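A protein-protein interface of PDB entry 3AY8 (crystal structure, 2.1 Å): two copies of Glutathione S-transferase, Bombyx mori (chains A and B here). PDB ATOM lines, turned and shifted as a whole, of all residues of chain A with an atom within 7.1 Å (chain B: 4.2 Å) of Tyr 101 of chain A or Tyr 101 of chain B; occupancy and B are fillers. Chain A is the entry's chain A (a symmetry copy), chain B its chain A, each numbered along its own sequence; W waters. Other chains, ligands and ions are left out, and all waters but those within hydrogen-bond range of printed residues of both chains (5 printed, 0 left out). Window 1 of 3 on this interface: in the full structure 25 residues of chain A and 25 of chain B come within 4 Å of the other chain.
The side-chain hydroxyl (OG) of Ser 104 of chain B sits at hydrogen-bond distance from the side-chain hydroxyl (OG) of Ser 104 of chain A.
The backbone NH of Trp 66 of chain A sits close to the side-chain amide nitrogen of Gln 98 of chain B, at 3.0 Å.
The backbone carbonyl oxygen (O) of Arg 69 of chain A lies within hydrogen-bond range of the side-chain sulfur (SG) of Cys 73 of chain A (3.3 Å).
The side-chain carboxylate of Glu 67 of chain B is in salt-bridge range of the guanidinium group of Arg 69 of chain B.
O of Tyr 101 of chain A lies within hydrogen-bond range of OG of Ser 104 of chain A (3.0 Å).
O of Tyr 101 of chain B sits at hydrogen-bond distance from OG of Ser 104 of chain B (3.0 Å).
Among the printed residues, merely in contact across the chains: Trp 66 of chain A with Phe 102 of chain B (3.98 Å), Glu 67 of chain A with Gln 98 of chain B (3.8 Å), Glu 67 of chain A with Tyr 101 of chain B (3.2 Å), Arg 69 of chain A with Tyr 101 of chain B (3.6 Å), Ala 70 of chain A with Gln 98 of chain B (3.8 Å), Ala 70 of chain A with Tyr 101 of chain B (3.9 Å), Ala 94 of chain A with Ala 70 of chain B (3.9 Å), Gln 98 of chain A with Glu 67 of chain B (3.8 Å), Gln 98 of chain A with Ala 70 of chain B (3.8 Å), Leu 100 of chain A with Tyr 101 of chain B (3.2 Å), Tyr 101 of chain A with Glu 67 of chain B (3.2 Å), Tyr 101 of chain A with Arg 69 of chain B (3.6 Å), Tyr 101 of chain A with Ala 70 of chain B (3.9 Å), Tyr 101 of chain A with Leu 100 of chain B (3.2 Å), Tyr 101 of chain A with Tyr 101 of chain B (3.3 Å), Tyr 101 of chain A with Ser 104 of chain B (3.7 Å), Ser 104 of chain A with Tyr 101 of chain B (3.7 Å), Ser 104 of chain A with Ala 105 of chain B (3.5 Å) and Ala 105 of chain A with Ser 104 of chain B (3.5 Å).
Printed residues of chain B within 4 Å of Tyr 101 of chain A: Glu 67, Arg 69, Ala 70, Leu 100, Tyr 101 and Ser 104.
Of the printed residues of chain B, Ser 104 of chain A touches Tyr 101 (3.7 Å), Ser 104 (2.7 Å) and Ala 105 (3.5 Å).
Printed residues of chain A within 4 Å of Leu 100 of chain B: Tyr 101 (3.2 Å).
Of the printed residues of chain A, Tyr 101 of chain B touches Glu 67 (3.2 Å), Arg 69 (3.6 Å), Ala 70 (3.9 Å), Leu 100 (3.2 Å), Tyr 101 (3.3 Å) and Ser 104 (3.7 Å).
Printed residues of chain B that touch a printed residue of chain A: Glu 67, Arg 69, Ala 70, Gln 98, Leu 100, Tyr 101, Phe 102, Ser 104 and Ala 105.
Hydrophobic or aromatic side chains of chain B that line the printed part of chain A: Ala 70, Leu 100, Tyr 101, Phe 102 and Ala 105.
Of the 23 printed residues of chain A, 10 touch a printed residue of chain B.
Along chain A the printed residues that touch a printed residue of chain B span positions 66 to 105.
Among the printed residues, 21 pairs touch across the chains.
Among the printed residues, no Asp or Glu carboxylate lies within 4 Å of a Lys or Arg side-chain nitrogen of the other chain.
Glu 67 of chain A touches Gln 98 of chain B, and with the chains exchanged Gln 98 of chain A touches Glu 67 of chain B.
Arg 69 of chain A touches Tyr 101 of chain B, and with the chains exchanged Tyr 101 of chain A touches Arg 69 of chain B.
Ala 70 of chain A touches Gln 98 of chain B, and with the chains exchanged Gln 98 of chain A touches Ala 70 of chain B.
Ser 104 of chain B touches its own counterpart, Ser 104 of chain A.
12 positions are printed for both chains.
Water W2 lies within hydrogen-bond range of OH of Tyr 101 of chain B (2.5 Å), OD1 of Asn 97 of chain A (3.0 Å) and SG of Cys 73 of chain A (3.2 Å).
Water W5 bridges the side-chain hydroxyl of Tyr 101 of chain A (2.5 Å) and the side-chain amide oxygen of Asn 97 of chain B (3.0 Å).
Water W3 lies within hydrogen-bond range of O of Ala 70 of chain B and ND2 of Asn 97 of chain A.
Water W4 bridges OH of Tyr 86 of chain A (2.9 Å) and ND2 of Asn 97 of chain B (2.9 Å).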
ATOM      1  N   TRP A  66     -17.762 -14.253  13.664  1.00  0.00           N
ATOM      2  CA  TRP A  66     -17.006 -15.063  14.609  1.00  0.00           C
ATOM      3  C   TRP A  66     -15.785 -14.288  15.098  1.00  0.00           C
ATOM      4  O   TRP A  66     -15.606 -13.113  14.739  1.00  0.00           O
ATOM      5  CB  TRP A  66     -16.661 -16.444  14.032  1.00  0.00           C
ATOM      6  CG  TRP A  66     -15.965 -16.413  12.701  1.00  0.00           C
ATOM      7  CD1 TRP A  66     -16.553 -16.348  11.472  1.00  0.00           C
ATOM      8  CD2 TRP A  66     -14.551 -16.462  12.468  1.00  0.00           C
ATOM      9  NE1 TRP A  66     -15.591 -16.348  10.481  1.00  0.00           N
ATOM     10  CE2 TRP A  66     -14.354 -16.421  11.069  1.00  0.00           C
ATOM     11  CE3 TRP A  66     -13.425 -16.552  13.306  1.00  0.00           C
ATOM     12  CZ2 TRP A  66     -13.075 -16.454  10.487  1.00  0.00           C
ATOM     13  CZ3 TRP A  66     -12.143 -16.578  12.718  1.00  0.00           C
ATOM     14  CH2 TRP A  66     -11.986 -16.530  11.329  1.00  0.00           C
ATOM     15  N   GLU A  67     -14.968 -14.966  15.911  1.00  0.00           N
ATOM     16  CA  GLU A  67     -13.815 -14.399  16.602  1.00  0.00           C
ATOM     17  C   GLU A  67     -14.274 -13.617  17.828  1.00  0.00           C
ATOM     18  O   GLU A  67     -14.843 -12.523  17.715  1.00  0.00           O
ATOM     19  CB  GLU A  67     -12.946 -13.540  15.674  1.00  0.00           C
ATOM     20  CG  GLU A  67     -11.474 -13.856  15.784  1.00  0.00           C
ATOM     21  CD  GLU A  67     -10.954 -13.729  17.205  1.00  0.00           C
ATOM     22  OE1 GLU A  67     -10.159 -14.593  17.629  1.00  0.00           O
ATOM     23  OE2 GLU A  67     -11.329 -12.761  17.900  1.00  0.00           O
ATOM     24  N   SER A  68     -14.019 -14.213  18.991  1.00  0.00           N
ATOM     25  CA  SER A  68     -14.514 -13.696  20.261  1.00  0.00           C
ATOM     26  C   SER A  68     -14.207 -12.217  20.490  1.00  0.00           C
ATOM     27  O   SER A  68     -15.062 -11.482  20.948  1.00  0.00           O
ATOM     28  CB  SER A  68     -13.980 -14.532  21.428  1.00  0.00           C
ATOM     29  OG  SER A  68     -12.588 -14.344  21.590  1.00  0.00           O
ATOM     30  N   ARG A  69     -12.996 -11.770  20.167  1.00  0.00           N
ATOM     31  CA  ARG A  69     -12.644 -10.374  20.462  1.00  0.00           C
ATOM     32  C   ARG A  69     -13.241  -9.364  19.469  1.00  0.00           C
ATOM     33  O   ARG A  69     -13.542  -8.240  19.852  1.00  0.00           O
ATOM     34  CB  ARG A  69     -11.131 -10.206  20.617  1.00  0.00           C
ATOM     35  CG  ARG A  69     -10.551 -11.085  21.748  1.00  0.00           C
ATOM     36  CD  ARG A  69      -9.220 -11.643  21.367  1.00  0.00           C
ATOM     37  NE  ARG A  69      -8.813 -12.795  22.181  1.00  0.00           N
ATOM     38  CZ  ARG A  69      -8.818 -14.064  21.778  1.00  0.00           C
ATOM     39  NH1 ARG A  69      -9.220 -14.395  20.569  1.00  0.00           N
ATOM     40  NH2 ARG A  69      -8.405 -15.018  22.600  1.00  0.00           N
ATOM     41  N   ALA A  70     -13.403  -9.773  18.213  1.00  0.00           N
ATOM     42  CA  ALA A  70     -14.188  -9.004  17.234  1.00  0.00           C
ATOM     43  C   ALA A  70     -15.647  -8.837  17.693  1.00  0.00           C
ATOM     44  O   ALA A  70     -16.216  -7.743  17.608  1.00  0.00           O
ATOM     45  CB  ALA A  70     -14.139  -9.669  15.886  1.00  0.00           C
ATOM     46  N   ILE A  71     -16.234  -9.930  18.182  1.00  0.00           N
ATOM     47  CA  ILE A  71     -17.578  -9.908  18.772  1.00  0.00           C
ATOM     48  C   ILE A  71     -17.660  -8.912  19.930  1.00  0.00           C
ATOM     49  O   ILE A  71     -18.546  -8.054  19.954  1.00  0.00           O
ATOM     50  CB  ILE A  71     -18.010 -11.334  19.222  1.00  0.00           C
ATOM     51  CG1 ILE A  71     -18.247 -12.211  17.994  1.00  0.00           C
ATOM     52  CG2 ILE A  71     -19.254 -11.286  20.126  1.00  0.00           C
ATOM     53  CD1 ILE A  71     -18.095 -13.721  18.266  1.00  0.00           C
ATOM     54  N   CYS A  73     -15.795  -6.272  20.657  1.00  0.00           N
ATOM     55  CA  CYS A  73     -15.684  -4.888  20.180  1.00  0.00           C
ATOM     56  C   CYS A  73     -16.946  -4.446  19.423  1.00  0.00           C
ATOM     57  O   CYS A  73     -17.372  -3.302  19.530  1.00  0.00           O
ATOM     58  CB  CYS A  73     -14.456  -4.725  19.269  1.00  0.00           C
ATOM     59  SG  CYS A  73     -12.870  -4.995  20.100  1.00  0.00           S
ATOM     60  N   TYR A  86     -15.386   0.021  26.164  1.00  0.00           N
ATOM     61  CA  TYR A  86     -14.525   0.101  24.981  1.00  0.00           C
ATOM     62  C   TYR A  86     -14.435   1.576  24.583  1.00  0.00           C
ATOM     63  O   TYR A  86     -15.194   2.026  23.736  1.00  0.00           O
ATOM     64  CB  TYR A  86     -15.121  -0.736  23.847  1.00  0.00           C
ATOM     65  CG  TYR A  86     -14.211  -0.997  22.660  1.00  0.00           C
ATOM     66  CD1 TYR A  86     -12.853  -1.298  22.836  1.00  0.00           C
ATOM     67  CD2 TYR A  86     -14.717  -0.982  21.367  1.00  0.00           C
ATOM     68  CE1 TYR A  86     -12.026  -1.549  21.748  1.00  0.00           C
ATOM     69  CE2 TYR A  86     -13.895  -1.233  20.265  1.00  0.00           C
ATOM     70  CZ  TYR A  86     -12.552  -1.519  20.470  1.00  0.00           C
ATOM     71  OH  TYR A  86     -11.737  -1.774  19.392  1.00  0.00           O
ATOM     72  N   ALA A  94      -6.776   2.099  21.640  1.00  0.00           N
ATOM     73  CA  ALA A  94      -5.562   1.390  21.219  1.00  0.00           C
ATOM     74  C   ALA A  94      -4.990   0.505  22.323  1.00  0.00           C
ATOM     75  O   ALA A  94      -4.528  -0.606  22.061  1.00  0.00           O
ATOM     76  CB  ALA A  94      -4.512   2.379  20.725  1.00  0.00           C
ATOM     77  N   VAL A  95      -5.054   0.980  23.562  1.00  0.00           N
ATOM     78  CA  VAL A  95      -4.589   0.188  24.684  1.00  0.00           C
ATOM     79  C   VAL A  95      -5.476  -1.035  24.919  1.00  0.00           C
ATOM     80  O   VAL A  95      -4.967  -2.127  25.152  1.00  0.00           O
ATOM     81  CB  VAL A  95      -4.393   1.039  25.967  1.00  0.00           C
ATOM     82  CG1 VAL A  95      -3.895   0.177  27.110  1.00  0.00           C
ATOM     83  CG2 VAL A  95      -3.357   2.162  25.697  1.00  0.00           C
ATOM     84  N   VAL A  96      -6.791  -0.865  24.849  1.00  0.00           N
ATOM     85  CA  VAL A  96      -7.696  -2.015  24.960  1.00  0.00           C
ATOM     86  C   VAL A  96      -7.445  -3.004  23.803  1.00  0.00           C
ATOM     87  O   VAL A  96      -7.371  -4.202  24.025  1.00  0.00           O
ATOM     88  CB  VAL A  96      -9.178  -1.578  24.991  1.00  0.00           C
ATOM     89  CG1 VAL A  96     -10.104  -2.790  24.898  1.00  0.00           C
ATOM     90  CG2 VAL A  96      -9.473  -0.762  26.258  1.00  0.00           C
ATOM     91  N   ASN A  97      -7.308  -2.498  22.578  1.00  0.00           N
ATOM     92  CA  ASN A  97      -7.045  -3.365  21.418  1.00  0.00           C
ATOM     93  C   ASN A  97      -5.752  -4.143  21.625  1.00  0.00           C
ATOM     94  O   ASN A  97      -5.674  -5.351  21.358  1.00  0.00           O
ATOM     95  CB  ASN A  97      -6.948  -2.547  20.130  1.00  0.00           C
ATOM     96  CG  ASN A  97      -8.308  -2.092  19.607  1.00  0.00           C
ATOM     97  OD1 ASN A  97      -9.365  -2.605  20.009  1.00  0.00           O
ATOM     98  ND2 ASN A  97      -8.283  -1.122  18.702  1.00  0.00           N
ATOM     99  N   GLN A  98      -4.764  -3.420  22.135  1.00  0.00           N
ATOM    100  CA  GLN A  98      -3.449  -3.975  22.444  1.00  0.00           C
ATOM    101  C   GLN A  98      -3.571  -5.156  23.408  1.00  0.00           C
ATOM    102  O   GLN A  98      -3.022  -6.229  23.138  1.00  0.00           O
ATOM    103  CB  GLN A  98      -2.533  -2.887  23.019  1.00  0.00           C
ATOM    104  CG  GLN A  98      -1.079  -3.269  23.199  1.00  0.00           C
ATOM    105  CD  GLN A  98      -0.370  -2.344  24.185  1.00  0.00           C
ATOM    106  OE1 GLN A  98      -0.614  -2.390  25.398  1.00  0.00           O
ATOM    107  NE2 GLN A  98       0.487  -1.493  23.669  1.00  0.00           N
ATOM    108  N   ARG A  99      -4.298  -4.974  24.520  1.00  0.00           N
ATOM    109  CA  ARG A  99      -4.488  -6.076  25.467  1.00  0.00           C
ATOM    110  C   ARG A  99      -5.284  -7.233  24.844  1.00  0.00           C
ATOM    111  O   ARG A  99      -5.028  -8.393  25.156  1.00  0.00           O
ATOM    112  CB  ARG A  99      -5.171  -5.614  26.774  1.00  0.00           C
ATOM    113  CG  ARG A  99      -4.540  -4.406  27.454  1.00  0.00           C
ATOM    114  CD  ARG A  99      -3.066  -4.530  27.767  1.00  0.00           C
ATOM    115  NE  ARG A  99      -2.709  -3.651  28.886  1.00  0.00           N
ATOM    116  CZ  ARG A  99      -1.605  -2.912  28.969  1.00  0.00           C
ATOM    117  NH1 ARG A  99      -0.716  -2.911  27.997  1.00  0.00           N
ATOM    118  NH2 ARG A  99      -1.391  -2.170  30.045  1.00  0.00           N
ATOM    119  N   LEU A 100      -6.244  -6.908  23.980  1.00  0.00           N
ATOM    120  CA  LEU A 100      -7.009  -7.938  23.262  1.00  0.00           C
ATOM    121  C   LEU A 100      -6.104  -8.752  22.358  1.00  0.00           C
ATOM    122  O   LEU A 100      -6.184  -9.977  22.358  1.00  0.00           O
ATOM    123  CB  LEU A 100      -8.183  -7.333  22.467  1.00  0.00           C
ATOM    124  CG  LEU A 100      -9.350  -6.794  23.316  1.00  0.00           C
ATOM    125  CD1 LEU A 100     -10.315  -5.929  22.475  1.00  0.00           C
ATOM    126  CD2 LEU A 100     -10.106  -7.944  24.019  1.00  0.00           C
ATOM    127  N   TYR A 101      -5.230  -8.085  21.601  1.00  0.00           N
ATOM    128  CA  TYR A 101      -4.281  -8.808  20.754  1.00  0.00           C
ATOM    129  C   TYR A 101      -3.278  -9.592  21.580  1.00  0.00           C
ATOM    130  O   TYR A 101      -2.904 -10.687  21.200  1.00  0.00           O
ATOM    131  CB  TYR A 101      -3.579  -7.891  19.729  1.00  0.00           C
ATOM    132  CG  TYR A 101      -4.518  -7.499  18.607  1.00  0.00           C
ATOM    133  CD1 TYR A 101      -4.931  -8.432  17.647  1.00  0.00           C
ATOM    134  CD2 TYR A 101      -5.027  -6.207  18.530  1.00  0.00           C
ATOM    135  CE1 TYR A 101      -5.821  -8.065  16.630  1.00  0.00           C
ATOM    136  CE2 TYR A 101      -5.910  -5.846  17.532  1.00  0.00           C
ATOM    137  CZ  TYR A 101      -6.304  -6.770  16.590  1.00  0.00           C
ATOM    138  OH  TYR A 101      -7.187  -6.372  15.608  1.00  0.00           O
ATOM    139  N   PHE A 102      -2.882  -9.051  22.732  1.00  0.00           N
ATOM    140  CA  PHE A 102      -2.083  -9.819  23.700  1.00  0.00           C
ATOM    141  C   PHE A 102      -2.811 -11.100  24.140  1.00  0.00           C
ATOM    142  O   PHE A 102      -2.208 -12.167  24.184  1.00  0.00           O
ATOM    143  CB  PHE A 102      -1.700  -8.923  24.886  1.00  0.00           C
ATOM    144  CG  PHE A 102      -1.125  -9.662  26.062  1.00  0.00           C
ATOM    145  CD1 PHE A 102       0.248  -9.916  26.143  1.00  0.00           C
ATOM    146  CD2 PHE A 102      -1.950 -10.094  27.096  1.00  0.00           C
ATOM    147  CE1 PHE A 102       0.773 -10.597  27.239  1.00  0.00           C
ATOM    148  CE2 PHE A 102      -1.419 -10.775  28.213  1.00  0.00           C
ATOM    149  CZ  PHE A 102      -0.067 -11.016  28.284  1.00  0.00           C
ATOM    150  N   ASP A 103      -4.110 -11.001  24.447  1.00  0.00           N
ATOM    151  CA  ASP A 103      -4.905 -12.181  24.780  1.00  0.00           C
ATOM    152  C   ASP A 103      -4.869 -13.214  23.630  1.00  0.00           C
ATOM    153  O   ASP A 103      -4.650 -14.405  23.856  1.00  0.00           O
ATOM    154  CB  ASP A 103      -6.367 -11.802  25.085  1.00  0.00           C
ATOM    155  CG  ASP A 103      -7.189 -12.991  25.544  1.00  0.00           C
ATOM    156  OD1 ASP A 103      -6.838 -13.595  26.582  1.00  0.00           O
ATOM    157  OD2 ASP A 103      -8.179 -13.337  24.869  1.00  0.00           O
ATOM    158  N   SER A 104      -5.076 -12.735  22.403  1.00  0.00           N
ATOM    159  CA  SER A 104      -5.242 -13.604  21.241  1.00  0.00           C
ATOM    160  C   SER A 104      -3.935 -14.185  20.720  1.00  0.00           C
ATOM    161  O   SER A 104      -3.921 -15.320  20.248  1.00  0.00           O
ATOM    162  CB  SER A 104      -5.940 -12.841  20.105  1.00  0.00           C
ATOM    163  OG  SER A 104      -5.054 -11.918  19.496  1.00  0.00           O
ATOM    164  N   ALA A 105      -2.852 -13.406  20.789  1.00  0.00           N
ATOM    165  CA  ALA A 105      -1.562 -13.803  20.200  1.00  0.00           C
ATOM    166  C   ALA A 105      -0.574 -14.435  21.179  1.00  0.00           C
ATOM    167  O   ALA A 105       0.363 -15.118  20.751  1.00  0.00           O
ATOM    168  CB  ALA A 105      -0.897 -12.599  19.507  1.00  0.00           C
ATOM    169  N   SER A 106      -0.741 -14.172  22.478  1.00  0.00           N
ATOM    170  CA  SER A 106       0.227 -14.661  23.479  1.00  0.00           C
ATOM    171  C   SER A 106      -0.437 -15.511  24.555  1.00  0.00           C
ATOM    172  O   SER A 106      -0.052 -16.655  24.773  1.00  0.00           O
ATOM    173  CB  SER A 106       0.963 -13.487  24.162  1.00  0.00           C
ATOM    174  OG  SER A 106       1.724 -12.767  23.222  1.00  0.00           O
ATOM    175  N   LEU A 107      -1.440 -14.948  25.215  1.00  0.00           N
ATOM    176  CA  LEU A 107      -2.011 -15.599  26.389  1.00  0.00           C
ATOM    177  C   LEU A 107      -2.769 -16.875  26.047  1.00  0.00           C
ATOM    178  O   LEU A 107      -2.379 -17.964  26.482  1.00  0.00           O
ATOM    179  CB  LEU A 107      -2.861 -14.629  27.219  1.00  0.00           C
ATOM    180  CG  LEU A 107      -3.507 -15.147  28.521  1.00  0.00           C
ATOM    181  CD1 LEU A 107      -2.499 -15.761  29.502  1.00  0.00           C
ATOM    182  CD2 LEU A 107      -4.267 -14.039  29.193  1.00  0.00           C
ATOM    183  N   ILE A 158     -13.601  -4.451  28.007  1.00  0.00           N
ATOM    184  CA  ILE A 158     -13.671  -5.749  27.345  1.00  0.00           C
ATOM    185  C   ILE A 158     -12.317  -6.474  27.289  1.00  0.00           C
ATOM    186  O   ILE A 158     -12.283  -7.679  27.065  1.00  0.00           O
ATOM    187  CB  ILE A 158     -14.315  -5.699  25.922  1.00  0.00           C
ATOM    188  CG1 ILE A 158     -13.488  -4.854  24.952  1.00  0.00           C
ATOM    189  CG2 ILE A 158     -15.778  -5.228  25.988  1.00  0.00           C
ATOM    190  CD1 ILE A 158     -13.990  -4.965  23.500  1.00  0.00           C
ATOM    191  N   GLU B  67       2.152  -3.934  19.804  1.00  0.00           N
ATOM    192  CA  GLU B  67       1.203  -4.831  19.155  1.00  0.00           C
ATOM    193  C   GLU B  67       0.860  -4.311  17.764  1.00  0.00           C
ATOM    194  O   GLU B  67       0.142  -3.313  17.611  1.00  0.00           O
ATOM    195  CB  GLU B  67      -0.056  -5.056  20.003  1.00  0.00           C
ATOM    196  CG  GLU B  67      -0.437  -6.513  20.118  1.00  0.00           C
ATOM    197  CD  GLU B  67      -0.628  -7.175  18.765  1.00  0.00           C
ATOM    198  OE1 GLU B  67      -0.181  -8.328  18.598  1.00  0.00           O
ATOM    199  OE2 GLU B  67      -1.232  -6.551  17.868  1.00  0.00           O
ATOM    200  N   ARG B  69      -1.091  -5.063  15.285  1.00  0.00           N
ATOM    201  CA  ARG B  69      -2.451  -4.822  14.783  1.00  0.00           C
ATOM    202  C   ARG B  69      -3.181  -3.677  15.502  1.00  0.00           C
ATOM    203  O   ARG B  69      -3.992  -2.993  14.889  1.00  0.00           O
ATOM    204  CB  ARG B  69      -3.274  -6.113  14.770  1.00  0.00           C
ATOM    205  CG  ARG B  69      -2.636  -7.212  13.891  1.00  0.00           C
ATOM    206  CD  ARG B  69      -2.794  -8.559  14.514  1.00  0.00           C
ATOM    207  NE  ARG B  69      -1.872  -9.566  13.975  1.00  0.00           N
ATOM    208  CZ  ARG B  69      -0.795 -10.039  14.599  1.00  0.00           C
ATOM    209  NH1 ARG B  69      -0.455  -9.607  15.795  1.00  0.00           N
ATOM    210  NH2 ARG B  69      -0.050 -10.967  14.015  1.00  0.00           N
ATOM    211  N   ALA B  70      -2.887  -3.481  16.785  1.00  0.00           N
ATOM    212  CA  ALA B  70      -3.317  -2.277  17.513  1.00  0.00           C
ATOM    213  C   ALA B  70      -2.746  -1.001  16.870  1.00  0.00           C
ATOM    214  O   ALA B  70      -3.461  -0.009  16.690  1.00  0.00           O
ATOM    215  CB  ALA B  70      -2.903  -2.364  18.957  1.00  0.00           C
ATOM    216  N   ASN B  97     -11.602  -6.501  11.879  1.00  0.00           N
ATOM    217  CA  ASN B  97     -11.087  -6.897  13.199  1.00  0.00           C
ATOM    218  C   ASN B  97     -10.968  -8.413  13.284  1.00  0.00           C
ATOM    219  O   ASN B  97      -9.967  -8.958  13.774  1.00  0.00           O
ATOM    220  CB  ASN B  97     -11.998  -6.394  14.320  1.00  0.00           C
ATOM    221  CG  ASN B  97     -11.837  -4.900  14.595  1.00  0.00           C
ATOM    222  OD1 ASN B  97     -10.856  -4.264  14.178  1.00  0.00           O
ATOM    223  ND2 ASN B  97     -12.805  -4.337  15.306  1.00  0.00           N
ATOM    224  N   GLN B  98     -12.000  -9.065  12.765  1.00  0.00           N
ATOM    225  CA  GLN B  98     -12.076 -10.522  12.712  1.00  0.00           C
ATOM    226  C   GLN B  98     -10.871 -11.102  11.971  1.00  0.00           C
ATOM    227  O   GLN B  98     -10.205 -12.003  12.492  1.00  0.00           O
ATOM    228  CB  GLN B  98     -13.391 -10.963  12.055  1.00  0.00           C
ATOM    229  CG  GLN B  98     -13.698 -12.444  12.112  1.00  0.00           C
ATOM    230  CD  GLN B  98     -14.727 -12.849  11.059  1.00  0.00           C
ATOM    231  OE1 GLN B  98     -14.439 -12.874   9.855  1.00  0.00           O
ATOM    232  NE2 GLN B  98     -15.928 -13.142  11.505  1.00  0.00           N
ATOM    233  N   ARG B  99     -10.574 -10.584  10.771  1.00  0.00           N
ATOM    234  CA  ARG B  99      -9.409 -11.067  10.025  1.00  0.00           C
ATOM    235  C   ARG B  99      -8.094 -10.754  10.756  1.00  0.00           C
ATOM    236  O   ARG B  99      -7.152 -11.539  10.690  1.00  0.00           O
ATOM    237  CB  ARG B  99      -9.357 -10.503   8.587  1.00  0.00           C
ATOM    238  CG  ARG B  99     -10.636 -10.660   7.774  1.00  0.00           C
ATOM    239  CD  ARG B  99     -11.165 -12.070   7.656  1.00  0.00           C
ATOM    240  NE  ARG B  99     -11.978 -12.209   6.443  1.00  0.00           N
ATOM    241  CZ  ARG B  99     -13.125 -12.877   6.351  1.00  0.00           C
ATOM    242  NH1 ARG B  99     -13.642 -13.484   7.400  1.00  0.00           N
ATOM    243  NH2 ARG B  99     -13.757 -12.940   5.188  1.00  0.00           N
ATOM    244  N   LEU B 100      -8.039  -9.607  11.432  1.00  0.00           N
ATOM    245  CA  LEU B 100      -6.861  -9.248  12.235  1.00  0.00           C
ATOM    246  C   LEU B 100      -6.658 -10.236  13.368  1.00  0.00           C
ATOM    247  O   LEU B 100      -5.541 -10.696  13.583  1.00  0.00           O
ATOM    248  CB  LEU B 100      -6.948  -7.805  12.771  1.00  0.00           C
ATOM    249  CG  LEU B 100      -6.795  -6.697  11.712  1.00  0.00           C
ATOM    250  CD1 LEU B 100      -7.211  -5.316  12.267  1.00  0.00           C
ATOM    251  CD2 LEU B 100      -5.356  -6.656  11.150  1.00  0.00           C
ATOM    252  N   TYR B 101      -7.731 -10.579  14.084  1.00  0.00           N
ATOM    253  CA  TYR B 101      -7.621 -11.576  15.150  1.00  0.00           C
ATOM    254  C   TYR B 101      -7.295 -12.952  14.598  1.00  0.00           C
ATOM    255  O   TYR B 101      -6.542 -13.687  15.212  1.00  0.00           O
ATOM    256  CB  TYR B 101      -8.866 -11.611  16.063  1.00  0.00           C
ATOM    257  CG  TYR B 101      -8.909 -10.408  16.982  1.00  0.00           C
ATOM    258  CD1 TYR B 101      -8.004 -10.273  18.043  1.00  0.00           C
ATOM    259  CD2 TYR B 101      -9.825  -9.385  16.765  1.00  0.00           C
ATOM    260  CE1 TYR B 101      -8.036  -9.143  18.871  1.00  0.00           C
ATOM    261  CE2 TYR B 101      -9.852  -8.267  17.575  1.00  0.00           C
ATOM    262  CZ  TYR B 101      -8.962  -8.148  18.619  1.00  0.00           C
ATOM    263  OH  TYR B 101      -9.020  -7.018  19.407  1.00  0.00           O
ATOM    264  N   PHE B 102      -7.824 -13.276  13.419  1.00  0.00           N
ATOM    265  CA  PHE B 102      -7.403 -14.491  12.703  1.00  0.00           C
ATOM    266  C   PHE B 102      -5.891 -14.484  12.425  1.00  0.00           C
ATOM    267  O   PHE B 102      -5.219 -15.487  12.644  1.00  0.00           O
ATOM    268  CB  PHE B 102      -8.235 -14.657  11.425  1.00  0.00           C
ATOM    269  CG  PHE B 102      -7.714 -15.699  10.474  1.00  0.00           C
ATOM    270  CD1 PHE B 102      -8.108 -17.035  10.596  1.00  0.00           C
ATOM    271  CD2 PHE B 102      -6.840 -15.347   9.450  1.00  0.00           C
ATOM    272  CE1 PHE B 102      -7.624 -17.994   9.708  1.00  0.00           C
ATOM    273  CE2 PHE B 102      -6.356 -16.314   8.543  1.00  0.00           C
ATOM    274  CZ  PHE B 102      -6.754 -17.624   8.670  1.00  0.00           C
ATOM    275  N   ASP B 103      -5.350 -13.351  11.961  1.00  0.00           N
ATOM    276  CA  ASP B 103      -3.908 -13.222  11.762  1.00  0.00           C
ATOM    277  C   ASP B 103      -3.142 -13.492  13.078  1.00  0.00           C
ATOM    278  O   ASP B 103      -2.166 -14.243  13.098  1.00  0.00           O
ATOM    279  CB  ASP B 103      -3.540 -11.824  11.231  1.00  0.00           C
ATOM    280  CG  ASP B 103      -2.064 -11.697  10.907  1.00  0.00           C
ATOM    281  OD1 ASP B 103      -1.576 -12.458  10.043  1.00  0.00           O
ATOM    282  OD2 ASP B 103      -1.382 -10.851  11.518  1.00  0.00           O
ATOM    283  N   SER B 104      -3.607 -12.878  14.166  1.00  0.00           N
ATOM    284  CA  SER B 104      -2.896 -12.897  15.441  1.00  0.00           C
ATOM    285  C   SER B 104      -3.038 -14.207  16.202  1.00  0.00           C
ATOM    286  O   SER B 104      -2.096 -14.626  16.871  1.00  0.00           O
ATOM    287  CB  SER B 104      -3.377 -11.743  16.333  1.00  0.00           C
ATOM    288  OG  SER B 104      -4.664 -12.014  16.859  1.00  0.00           O
ATOM    289  N   ALA B 105      -4.213 -14.838  16.113  1.00  0.00           N
ATOM    290  CA  ALA B 105      -4.518 -16.041  16.906  1.00  0.00           C
ATOM    291  C   ALA B 105      -4.302 -17.365  16.176  1.00  0.00           C
ATOM    292  O   ALA B 105      -4.175 -18.410  16.824  1.00  0.00           O
ATOM    293  CB  ALA B 105      -5.962 -15.979  17.439  1.00  0.00           C
HETATM  294  O   HOH W   1     -15.356  -5.746  15.935  1.00  0.00           O
HETATM  295  O   HOH W   2     -10.174  -5.022  18.370  1.00  0.00           O
HETATM  296  O   HOH W   3      -5.804   0.403  18.057  1.00  0.00           O
HETATM  297  O   HOH W   4     -13.295  -1.945  16.921  1.00  0.00           O
HETATM  298  O   HOH W   5      -8.537  -4.300  16.129  1.00  0.00           O
